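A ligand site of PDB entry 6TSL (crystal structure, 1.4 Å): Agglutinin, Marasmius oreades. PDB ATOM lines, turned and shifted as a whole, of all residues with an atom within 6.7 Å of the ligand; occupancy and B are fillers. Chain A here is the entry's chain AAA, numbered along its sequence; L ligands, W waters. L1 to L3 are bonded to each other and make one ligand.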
ATOM      1  N   HIS A   9     -30.915  -1.970 -11.464  1.00  0.00           N
ATOM      2  CA  HIS A   9     -30.798  -0.828 -10.550  1.00  0.00           C
ATOM      3  C   HIS A   9     -30.924  -1.343  -9.121  1.00  0.00           C
ATOM      4  O   HIS A   9     -31.939  -1.961  -8.825  1.00  0.00           O
ATOM      5  CB  HIS A   9     -31.859   0.206 -10.893  1.00  0.00           C
ATOM      6  CG  HIS A   9     -31.654   1.527 -10.234  1.00  0.00           C
ATOM      7  ND1 HIS A   9     -32.548   2.037  -9.298  1.00  0.00           N
ATOM      8  CD2 HIS A   9     -30.638   2.426 -10.313  1.00  0.00           C
ATOM      9  CE1 HIS A   9     -32.092   3.197  -8.860  1.00  0.00           C
ATOM     10  NE2 HIS A   9     -30.944   3.464  -9.499  1.00  0.00           N
ATOM     11  N   ASP A  20     -24.035   3.126  -6.551  1.00  0.00           N
ATOM     12  CA  ASP A  20     -23.645   4.198  -7.489  1.00  0.00           C
ATOM     13  C   ASP A  20     -22.115   4.162  -7.652  1.00  0.00           C
ATOM     14  O   ASP A  20     -21.409   4.161  -6.635  1.00  0.00           O
ATOM     15  CB  ASP A  20     -24.153   5.544  -6.994  1.00  0.00           C
ATOM     16  CG  ASP A  20     -23.886   6.725  -7.920  1.00  0.00           C
ATOM     17  OD1 ASP A  20     -22.690   7.060  -8.101  1.00  0.00           O
ATOM     18  OD2 ASP A  20     -24.901   7.429  -8.294  1.00  0.00           O
ATOM     19  N   LEU A  21     -21.617   4.073  -8.874  1.00  0.00           N
ATOM     20  CA  LEU A  21     -20.164   4.241  -9.132  1.00  0.00           C
ATOM     21  C   LEU A  21     -19.863   5.739  -9.205  1.00  0.00           C
ATOM     22  O   LEU A  21     -20.391   6.399 -10.140  1.00  0.00           O
ATOM     23  CB  LEU A  21     -19.790   3.543 -10.434  1.00  0.00           C
ATOM     24  CG  LEU A  21     -18.307   3.629 -10.797  1.00  0.00           C
ATOM     25  CD1 LEU A  21     -17.445   2.951  -9.763  1.00  0.00           C
ATOM     26  CD2 LEU A  21     -18.051   3.015 -12.170  1.00  0.00           C
ATOM     27  N   LYS A  22     -19.116   6.267  -8.249  1.00  0.00           N
ATOM     28  CA  LYS A  22     -19.091   7.727  -8.031  1.00  0.00           C
ATOM     29  C   LYS A  22     -18.586   8.436  -9.317  1.00  0.00           C
ATOM     30  O   LYS A  22     -17.471   8.104  -9.799  1.00  0.00           O
ATOM     31  CB  LYS A  22     -18.214   8.085  -6.827  1.00  0.00           C
ATOM     32  CG  LYS A  22     -18.561   9.406  -6.209  1.00  0.00           C
ATOM     33  CD  LYS A  22     -17.792   9.745  -4.992  1.00  0.00           C
ATOM     34  CE  LYS A  22     -18.116  11.142  -4.486  1.00  0.00           C
ATOM     35  NZ  LYS A  22     -17.644  11.335  -3.091  1.00  0.00           N
ATOM     36  N   ASP A  23     -19.358   9.401  -9.796  1.00  0.00           N
ATOM     37  CA  ASP A  23     -19.072  10.228 -10.993  1.00  0.00           C
ATOM     38  C   ASP A  23     -18.946   9.328 -12.247  1.00  0.00           C
ATOM     39  O   ASP A  23     -18.500   9.829 -13.285  1.00  0.00           O
ATOM     40  CB  ASP A  23     -17.804  11.058 -10.807  1.00  0.00           C
ATOM     41  CG  ASP A  23     -17.788  12.320 -11.662  1.00  0.00           C
ATOM     42  OD1 ASP A  23     -18.878  12.890 -11.886  1.00  0.00           O
ATOM     43  OD2 ASP A  23     -16.708  12.666 -12.183  1.00  0.00           O
ATOM     44  N   GLY A  24     -19.359   8.072 -12.150  1.00  0.00           N
ATOM     45  CA  GLY A  24     -19.289   7.139 -13.283  1.00  0.00           C
ATOM     46  C   GLY A  24     -17.836   6.880 -13.730  1.00  0.00           C
ATOM     47  O   GLY A  24     -17.652   6.433 -14.866  1.00  0.00           O
ATOM     48  N   VAL A  33     -20.760   3.836  -3.899  1.00  0.00           N
ATOM     49  CA  VAL A  33     -21.380   4.570  -2.762  1.00  0.00           C
ATOM     50  C   VAL A  33     -22.901   4.446  -2.865  1.00  0.00           C
ATOM     51  O   VAL A  33     -23.421   4.199  -3.987  1.00  0.00           O
ATOM     52  CB  VAL A  33     -20.940   6.054  -2.765  1.00  0.00           C
ATOM     53  CG1 VAL A  33     -19.449   6.192  -2.503  1.00  0.00           C
ATOM     54  CG2 VAL A  33     -21.323   6.759  -4.060  1.00  0.00           C
ATOM     55  N   TRP A  35     -26.422   6.454  -3.154  1.00  0.00           N
ATOM     56  CA  TRP A  35     -26.835   7.746  -3.776  1.00  0.00           C
ATOM     57  C   TRP A  35     -28.311   7.701  -4.078  1.00  0.00           C
ATOM     58  O   TRP A  35     -28.788   6.644  -4.501  1.00  0.00           O
ATOM     59  CB  TRP A  35     -26.004   8.031  -5.049  1.00  0.00           C
ATOM     60  CG  TRP A  35     -25.846   9.490  -5.359  1.00  0.00           C
ATOM     61  CD1 TRP A  35     -26.772  10.327  -5.922  1.00  0.00           C
ATOM     62  CD2 TRP A  35     -24.683  10.299  -5.089  1.00  0.00           C
ATOM     63  NE1 TRP A  35     -26.265  11.605  -5.994  1.00  0.00           N
ATOM     64  CE2 TRP A  35     -24.996  11.612  -5.501  1.00  0.00           C
ATOM     65  CE3 TRP A  35     -23.432  10.043  -4.510  1.00  0.00           C
ATOM     66  CZ2 TRP A  35     -24.072  12.660  -5.368  1.00  0.00           C
ATOM     67  CZ3 TRP A  35     -22.532  11.071  -4.382  1.00  0.00           C
ATOM     68  CH2 TRP A  35     -22.845  12.363  -4.806  1.00  0.00           C
ATOM     69  N   GLN A  36     -28.989   8.813  -3.963  1.00  0.00           N
ATOM     70  CA  GLN A  36     -30.430   8.885  -4.250  1.00  0.00           C
ATOM     71  C   GLN A  36     -30.656   8.765  -5.765  1.00  0.00           C
ATOM     72  O   GLN A  36     -29.680   8.907  -6.522  1.00  0.00           O
ATOM     73  CB  GLN A  36     -31.037  10.196  -3.692  1.00  0.00           C
ATOM     74  CG  GLN A  36     -30.538  11.465  -4.363  1.00  0.00           C
ATOM     75  CD  GLN A  36     -31.203  12.704  -3.799  1.00  0.00           C
ATOM     76  OE1 GLN A  36     -32.417  12.880  -3.913  1.00  0.00           O
ATOM     77  NE2 GLN A  36     -30.435  13.527  -3.120  1.00  0.00           N
ATOM     78  N   PHE A  37     -31.875   8.510  -6.169  1.00  0.00           N
ATOM     79  CA  PHE A  37     -32.184   8.198  -7.580  1.00  0.00           C
ATOM     80  C   PHE A  37     -33.548   8.744  -7.937  1.00  0.00           C
ATOM     81  O   PHE A  37     -34.301   9.151  -7.041  1.00  0.00           O
ATOM     82  CB  PHE A  37     -32.102   6.684  -7.796  1.00  0.00           C
ATOM     83  CG  PHE A  37     -32.997   5.855  -6.913  1.00  0.00           C
ATOM     84  CD1 PHE A  37     -34.271   5.493  -7.324  1.00  0.00           C
ATOM     85  CD2 PHE A  37     -32.530   5.328  -5.712  1.00  0.00           C
ATOM     86  CE1 PHE A  37     -35.070   4.692  -6.525  1.00  0.00           C
ATOM     87  CE2 PHE A  37     -33.319   4.501  -4.934  1.00  0.00           C
ATOM     88  CZ  PHE A  37     -34.602   4.223  -5.319  1.00  0.00           C
ATOM     89  N   THR A  38     -33.786   8.886  -9.218  1.00  0.00           N
ATOM     90  CA  THR A  38     -35.084   9.319  -9.769  1.00  0.00           C
ATOM     91  C   THR A  38     -35.685   8.161 -10.533  1.00  0.00           C
ATOM     92  O   THR A  38     -35.139   7.745 -11.543  1.00  0.00           O
ATOM     93  CB  THR A  38     -34.923  10.560 -10.665  1.00  0.00           C
ATOM     94  OG1 THR A  38     -34.084  11.517  -9.984  1.00  0.00           O
ATOM     95  CG2 THR A  38     -36.247  11.188 -11.021  1.00  0.00           C
ATOM     96  N   PRO A  39     -36.799   7.583 -10.057  1.00  0.00           N
ATOM     97  CA  PRO A  39     -37.510   6.552 -10.826  1.00  0.00           C
ATOM     98  C   PRO A  39     -37.917   7.032 -12.236  1.00  0.00           C
ATOM     99  O   PRO A  39     -38.074   8.248 -12.430  1.00  0.00           O
ATOM    100  CB  PRO A  39     -38.753   6.245  -9.960  1.00  0.00           C
ATOM    101  CG  PRO A  39     -38.291   6.557  -8.537  1.00  0.00           C
ATOM    102  CD  PRO A  39     -37.334   7.730  -8.693  1.00  0.00           C
ATOM    103  N   THR A  41     -36.250   7.304 -14.929  1.00  0.00           N
ATOM    104  CA  THR A  41     -35.156   7.941 -15.677  1.00  0.00           C
ATOM    105  C   THR A  41     -34.100   6.900 -15.954  1.00  0.00           C
ATOM    106  O   THR A  41     -34.100   5.868 -15.250  1.00  0.00           O
ATOM    107  CB  THR A  41     -34.544   9.138 -14.898  1.00  0.00           C
ATOM    108  OG1 THR A  41     -33.779   8.636 -13.793  1.00  0.00           O
ATOM    109  CG2 THR A  41     -35.569  10.110 -14.399  1.00  0.00           C
ATOM    110  N   ILE A  42     -33.133   7.247 -16.766  1.00  0.00           N
ATOM    111  CA  ILE A  42     -31.821   6.582 -16.771  1.00  0.00           C
ATOM    112  C   ILE A  42     -30.990   7.143 -15.617  1.00  0.00           C
ATOM    113  O   ILE A  42     -30.717   8.376 -15.635  1.00  0.00           O
ATOM    114  CB  ILE A  42     -31.124   6.773 -18.123  1.00  0.00           C
ATOM    115  CG1 ILE A  42     -31.933   6.137 -19.259  1.00  0.00           C
ATOM    116  CG2 ILE A  42     -29.705   6.233 -18.060  1.00  0.00           C
ATOM    117  CD1 ILE A  42     -32.157   4.661 -19.102  1.00  0.00           C
ATOM    118  N   ASN A  43     -30.716   6.331 -14.620  1.00  0.00           N
ATOM    119  CA  ASN A  43     -29.769   6.690 -13.528  1.00  0.00           C
ATOM    120  C   ASN A  43     -28.354   6.296 -13.951  1.00  0.00           C
ATOM    121  O   ASN A  43     -27.994   5.110 -13.825  1.00  0.00           O
ATOM    122  CB  ASN A  43     -30.199   6.069 -12.193  1.00  0.00           C
ATOM    123  CG  ASN A  43     -31.478   6.680 -11.650  1.00  0.00           C
ATOM    124  OD1 ASN A  43     -31.473   7.792 -11.130  1.00  0.00           O
ATOM    125  ND2 ASN A  43     -32.607   6.009 -11.884  1.00  0.00           N
ATOM    126  N   TRP A  44     -27.640   7.235 -14.567  1.00  0.00           N
ATOM    127  CA  TRP A  44     -26.499   6.974 -15.476  1.00  0.00           C
ATOM    128  C   TRP A  44     -25.407   6.162 -14.755  1.00  0.00           C
ATOM    129  O   TRP A  44     -24.700   5.449 -15.430  1.00  0.00           O
ATOM    130  CB  TRP A  44     -25.958   8.290 -16.026  1.00  0.00           C
ATOM    131  CG  TRP A  44     -26.744   8.810 -17.163  1.00  0.00           C
ATOM    132  CD1 TRP A  44     -27.760   9.727 -17.124  1.00  0.00           C
ATOM    133  CD2 TRP A  44     -26.666   8.348 -18.519  1.00  0.00           C
ATOM    134  NE1 TRP A  44     -28.308   9.873 -18.369  1.00  0.00           N
ATOM    135  CE2 TRP A  44     -27.636   9.073 -19.240  1.00  0.00           C
ATOM    136  CE3 TRP A  44     -25.881   7.420 -19.182  1.00  0.00           C
ATOM    137  CZ2 TRP A  44     -27.806   8.894 -20.609  1.00  0.00           C
ATOM    138  CZ3 TRP A  44     -26.058   7.253 -20.530  1.00  0.00           C
ATOM    139  CH2 TRP A  44     -27.034   7.953 -21.224  1.00  0.00           C
ATOM    140  N   HIS A  45     -25.202   6.404 -13.456  1.00  0.00           N
ATOM    141  CA  HIS A  45     -24.038   5.821 -12.735  1.00  0.00           C
ATOM    142  C   HIS A  45     -24.469   4.612 -11.897  1.00  0.00           C
ATOM    143  O   HIS A  45     -23.606   4.059 -11.177  1.00  0.00           O
ATOM    144  CB  HIS A  45     -23.334   6.891 -11.892  1.00  0.00           C
ATOM    145  CG  HIS A  45     -22.887   8.079 -12.669  1.00  0.00           C
ATOM    146  ND1 HIS A  45     -22.615   9.310 -12.059  1.00  0.00           N
ATOM    147  CD2 HIS A  45     -22.570   8.234 -13.989  1.00  0.00           C
ATOM    148  CE1 HIS A  45     -22.216  10.188 -12.991  1.00  0.00           C
ATOM    149  NE2 HIS A  45     -22.160   9.566 -14.171  1.00  0.00           N
ATOM    150  N   GLN A  46     -25.700   4.147 -12.067  1.00  0.00           N
ATOM    151  CA  GLN A  46     -26.360   3.239 -11.074  1.00  0.00           C
ATOM    152  C   GLN A  46     -26.902   1.976 -11.778  1.00  0.00           C
ATOM    153  O   GLN A  46     -27.775   1.328 -11.190  1.00  0.00           O
ATOM    154  CB  GLN A  46     -27.476   3.967 -10.345  1.00  0.00           C
ATOM    155  CG  GLN A  46     -27.015   5.233  -9.643  1.00  0.00           C
ATOM    156  CD  GLN A  46     -28.109   5.928  -8.874  1.00  0.00           C
ATOM    157  OE1 GLN A  46     -29.303   5.622  -9.005  1.00  0.00           O
ATOM    158  NE2 GLN A  46     -27.711   6.964  -8.129  1.00  0.00           N
ATOM    159  N   PHE A  66     -22.146   2.219 -17.456  1.00  0.00           N
ATOM    160  CA  PHE A  66     -21.585   3.500 -17.945  1.00  0.00           C
ATOM    161  C   PHE A  66     -20.046   3.370 -18.074  1.00  0.00           C
ATOM    162  O   PHE A  66     -19.506   3.676 -19.135  1.00  0.00           O
ATOM    163  CB  PHE A  66     -21.976   4.643 -17.034  1.00  0.00           C
ATOM    164  CG  PHE A  66     -21.474   5.988 -17.476  1.00  0.00           C
ATOM    165  CD1 PHE A  66     -22.115   6.684 -18.495  1.00  0.00           C
ATOM    166  CD2 PHE A  66     -20.344   6.542 -16.917  1.00  0.00           C
ATOM    167  CE1 PHE A  66     -21.646   7.924 -18.900  1.00  0.00           C
ATOM    168  CE2 PHE A  66     -19.874   7.783 -17.332  1.00  0.00           C
ATOM    169  CZ  PHE A  66     -20.529   8.459 -18.325  1.00  0.00           C
ATOM    170  N   ASP A 131     -26.015  11.110   0.199  1.00  0.00           N
ATOM    171  CA  ASP A 131     -25.361  10.933  -1.129  1.00  0.00           C
ATOM    172  C   ASP A 131     -23.860  10.792  -0.930  1.00  0.00           C
ATOM    173  O   ASP A 131     -23.252  11.690  -0.328  1.00  0.00           O
ATOM    174  CB  ASP A 131     -25.699  12.090  -2.055  1.00  0.00           C
ATOM    175  CG  ASP A 131     -27.140  12.119  -2.499  1.00  0.00           C
ATOM    176  OD1 ASP A 131     -27.810  11.035  -2.425  1.00  0.00           O
ATOM    177  OD2 ASP A 131     -27.607  13.190  -2.883  1.00  0.00           O
HETATM  178  C1  LIG L   1     -26.960  13.094 -12.553  1.00  0.00           C
HETATM  179  C2  LIG L   1     -27.497  14.469 -12.943  1.00  0.00           C
HETATM  180  C3  LIG L   1     -26.475  15.239 -13.802  1.00  0.00           C
HETATM  181  C4  LIG L   1     -26.011  14.387 -14.942  1.00  0.00           C
HETATM  182  C5  LIG L   1     -25.450  13.070 -14.422  1.00  0.00           C
HETATM  183  C6  LIG L   1     -24.995  12.171 -15.526  1.00  0.00           C
HETATM  184  O1  LIG L   1     -27.820  15.177 -11.744  1.00  0.00           O
HETATM  185  O2  LIG L   1     -27.082  16.448 -14.287  1.00  0.00           O
HETATM  186  O3  LIG L   1     -27.114  14.106 -15.869  1.00  0.00           O
HETATM  187  O4  LIG L   1     -26.477  12.385 -13.698  1.00  0.00           O
HETATM  188  C1  LG2 L   2     -23.767  12.699 -10.807  1.00  0.00           C
HETATM  189  C2  LG2 L   2     -25.171  12.178 -11.140  1.00  0.00           C
HETATM  190  C3  LG2 L   2     -25.866  11.629  -9.909  1.00  0.00           C
HETATM  191  C4  LG2 L   2     -24.972  10.631  -9.192  1.00  0.00           C
HETATM  192  C5  LG2 L   2     -23.597  11.266  -8.935  1.00  0.00           C
HETATM  193  C6  LG2 L   2     -22.624  10.359  -8.199  1.00  0.00           C
HETATM  194  O1  LG2 L   2     -23.146  13.061 -11.994  1.00  0.00           O
HETATM  195  O2  LG2 L   2     -25.936  13.257 -11.689  1.00  0.00           O
HETATM  196  O3  LG2 L   2     -27.163  11.042 -10.312  1.00  0.00           O
HETATM  197  O4  LG2 L   2     -24.823   9.423  -9.971  1.00  0.00           O
HETATM  198  O5  LG2 L   2     -23.016  11.665 -10.195  1.00  0.00           O
HETATM  199  O6  LG2 L   2     -22.098   9.342  -9.079  1.00  0.00           O
HETATM  200  C1  LG3 L   3     -27.993  10.555  -9.370  1.00  0.00           C
HETATM  201  C2  LG3 L   3     -29.355  10.068  -9.916  1.00  0.00           C
HETATM  202  C3  LG3 L   3     -30.216  11.263 -10.317  1.00  0.00           C
HETATM  203  C4  LG3 L   3     -30.282  12.247  -9.149  1.00  0.00           C
HETATM  204  C5  LG3 L   3     -28.885  12.669  -8.765  1.00  0.00           C
HETATM  205  C6  LG3 L   3     -28.850  13.715  -7.627  1.00  0.00           C
HETATM  206  O1  LG3 L   3     -29.153   9.217 -11.033  1.00  0.00           O
HETATM  207  O2  LG3 L   3     -31.513  10.813 -10.689  1.00  0.00           O
HETATM  208  O3  LG3 L   3     -30.981  11.636  -8.025  1.00  0.00           O
HETATM  209  O4  LG3 L   3     -28.177  11.516  -8.342  1.00  0.00           O
HETATM  210  O5  LG3 L   3     -27.466  14.108  -7.299  1.00  0.00           O
HETATM  211  O   HOH W   1     -31.522  10.209 -13.307  1.00  0.00           O
HETATM  212  O   HOH W   2     -26.733  14.960  -4.826  1.00  0.00           O
HETATM  213  O   HOH W   3     -28.634  10.104 -13.793  1.00  0.00           O
HETATM  214  O   HOH W   4     -29.353  12.526 -15.226  1.00  0.00           O
HETATM  215  O   HOH W   5     -30.442  15.008 -11.009  1.00  0.00           O
HETATM  216  O   HOH W   6     -26.278  15.489  -9.391  1.00  0.00           O
HETATM  217  O   HOH W   7     -26.639   8.189 -11.641  1.00  0.00           O
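Merely in contact with the ligand: Leu 21 (3.6 Å), Lys 22 (3.6 Å), Phe 37 (3.7 Å) and Gln 46 (3.8 Å). Hydrophobic or aromatic side chains within 4 Å of the ligand: Trp 35 and His 45. 11 residues have an atom within 4 Å of the ligand: Asp 20, Leu 21, Lys 22, Asp 23, Trp 35, Gln 36, Phe 37, Thr 38, Asn 43, His 45 and Gln 46. The nearest printed residue that does not touch the ligand is Trp 44 (4.02 Å).
NE2 of Gln 46 is in hydrogen-bond range of OD2 of Asp 20 (2.9 Å). N of Val 33 is in hydrogen-bond range of O of Asp 20, at 2.8 Å. ND2 of Asn 43 lies within hydrogen-bond range of O of Thr 38. The side-chain hydroxyl (OG1) of Thr 41 sits at hydrogen-bond distance from the side-chain amide nitrogen (ND2) of Asn 43, 3.5 Å away. The backbone carbonyl oxygen (O) of Thr 38 lies within hydrogen-bond range of the side-chain hydroxyl (OG1) of Thr 41 (2.8 Å). A ring nitrogen (ND1) of His 45 sits at hydrogen-bond distance from the backbone NH (N) of Gly 24. NE2 of Gln 36 lies within hydrogen-bond range of OD2 of Asp 131 (2.9 Å). The side-chain amide oxygen of Gln 46 is in hydrogen-bond range of a ring nitrogen (NE2) of His 9, 2.8 Å away.
The side-chain carboxylate (OD1) of Asp 20 lies within hydrogen-bond range of an oxygen (O6) of LG2 L2 (2.6 Å). O1 of LG3 L3 is in hydrogen-bond range of OD1 of Asn 43, at 2.7 Å. N of Thr 38 lies within hydrogen-bond range of O2 of LG3 L3 (3.3 Å). OG1 of Thr 38 is in hydrogen-bond range of O2 of LG3 L3, at 2.8 Å. O6 of LG2 L2 lies within hydrogen-bond range of N of Asp 23 (2.8 Å). An oxygen (O6) of LG2 L2 sits at hydrogen-bond distance from a ring nitrogen (ND1) of His 45, at 3.0 Å. The indole nitrogen (NE1) of Trp 35 sits at hydrogen-bond distance from an oxygen (O4) of LG3 L3, at 3.0 Å. O3 of LG3 L3 is in hydrogen-bond range of O of Gln 36 (3.4 Å).
Water W1 lies within hydrogen-bond range of O2 of LG3 L3 (2.7 Å), OG1 of Thr 41 (2.8 Å), O of Ile 42 (3.1 Å) and OD1 of Asn 43 (3.3 Å). Water W2 lies within hydrogen-bond range of O5 of LG3 L3 and OD2 of Asp 131. Water W7 lies within hydrogen-bond range of an oxygen (O4) of LG2 L2 (2.8 Å), the backbone NH of His 45 (2.9 Å) and the backbone NH of Trp 44 (3.2 Å). Water W3 lies within hydrogen-bond range of an oxygen (O1) of LG3 L3, the backbone NH of Trp 44 and the backbone carbonyl oxygen of Ile 42.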
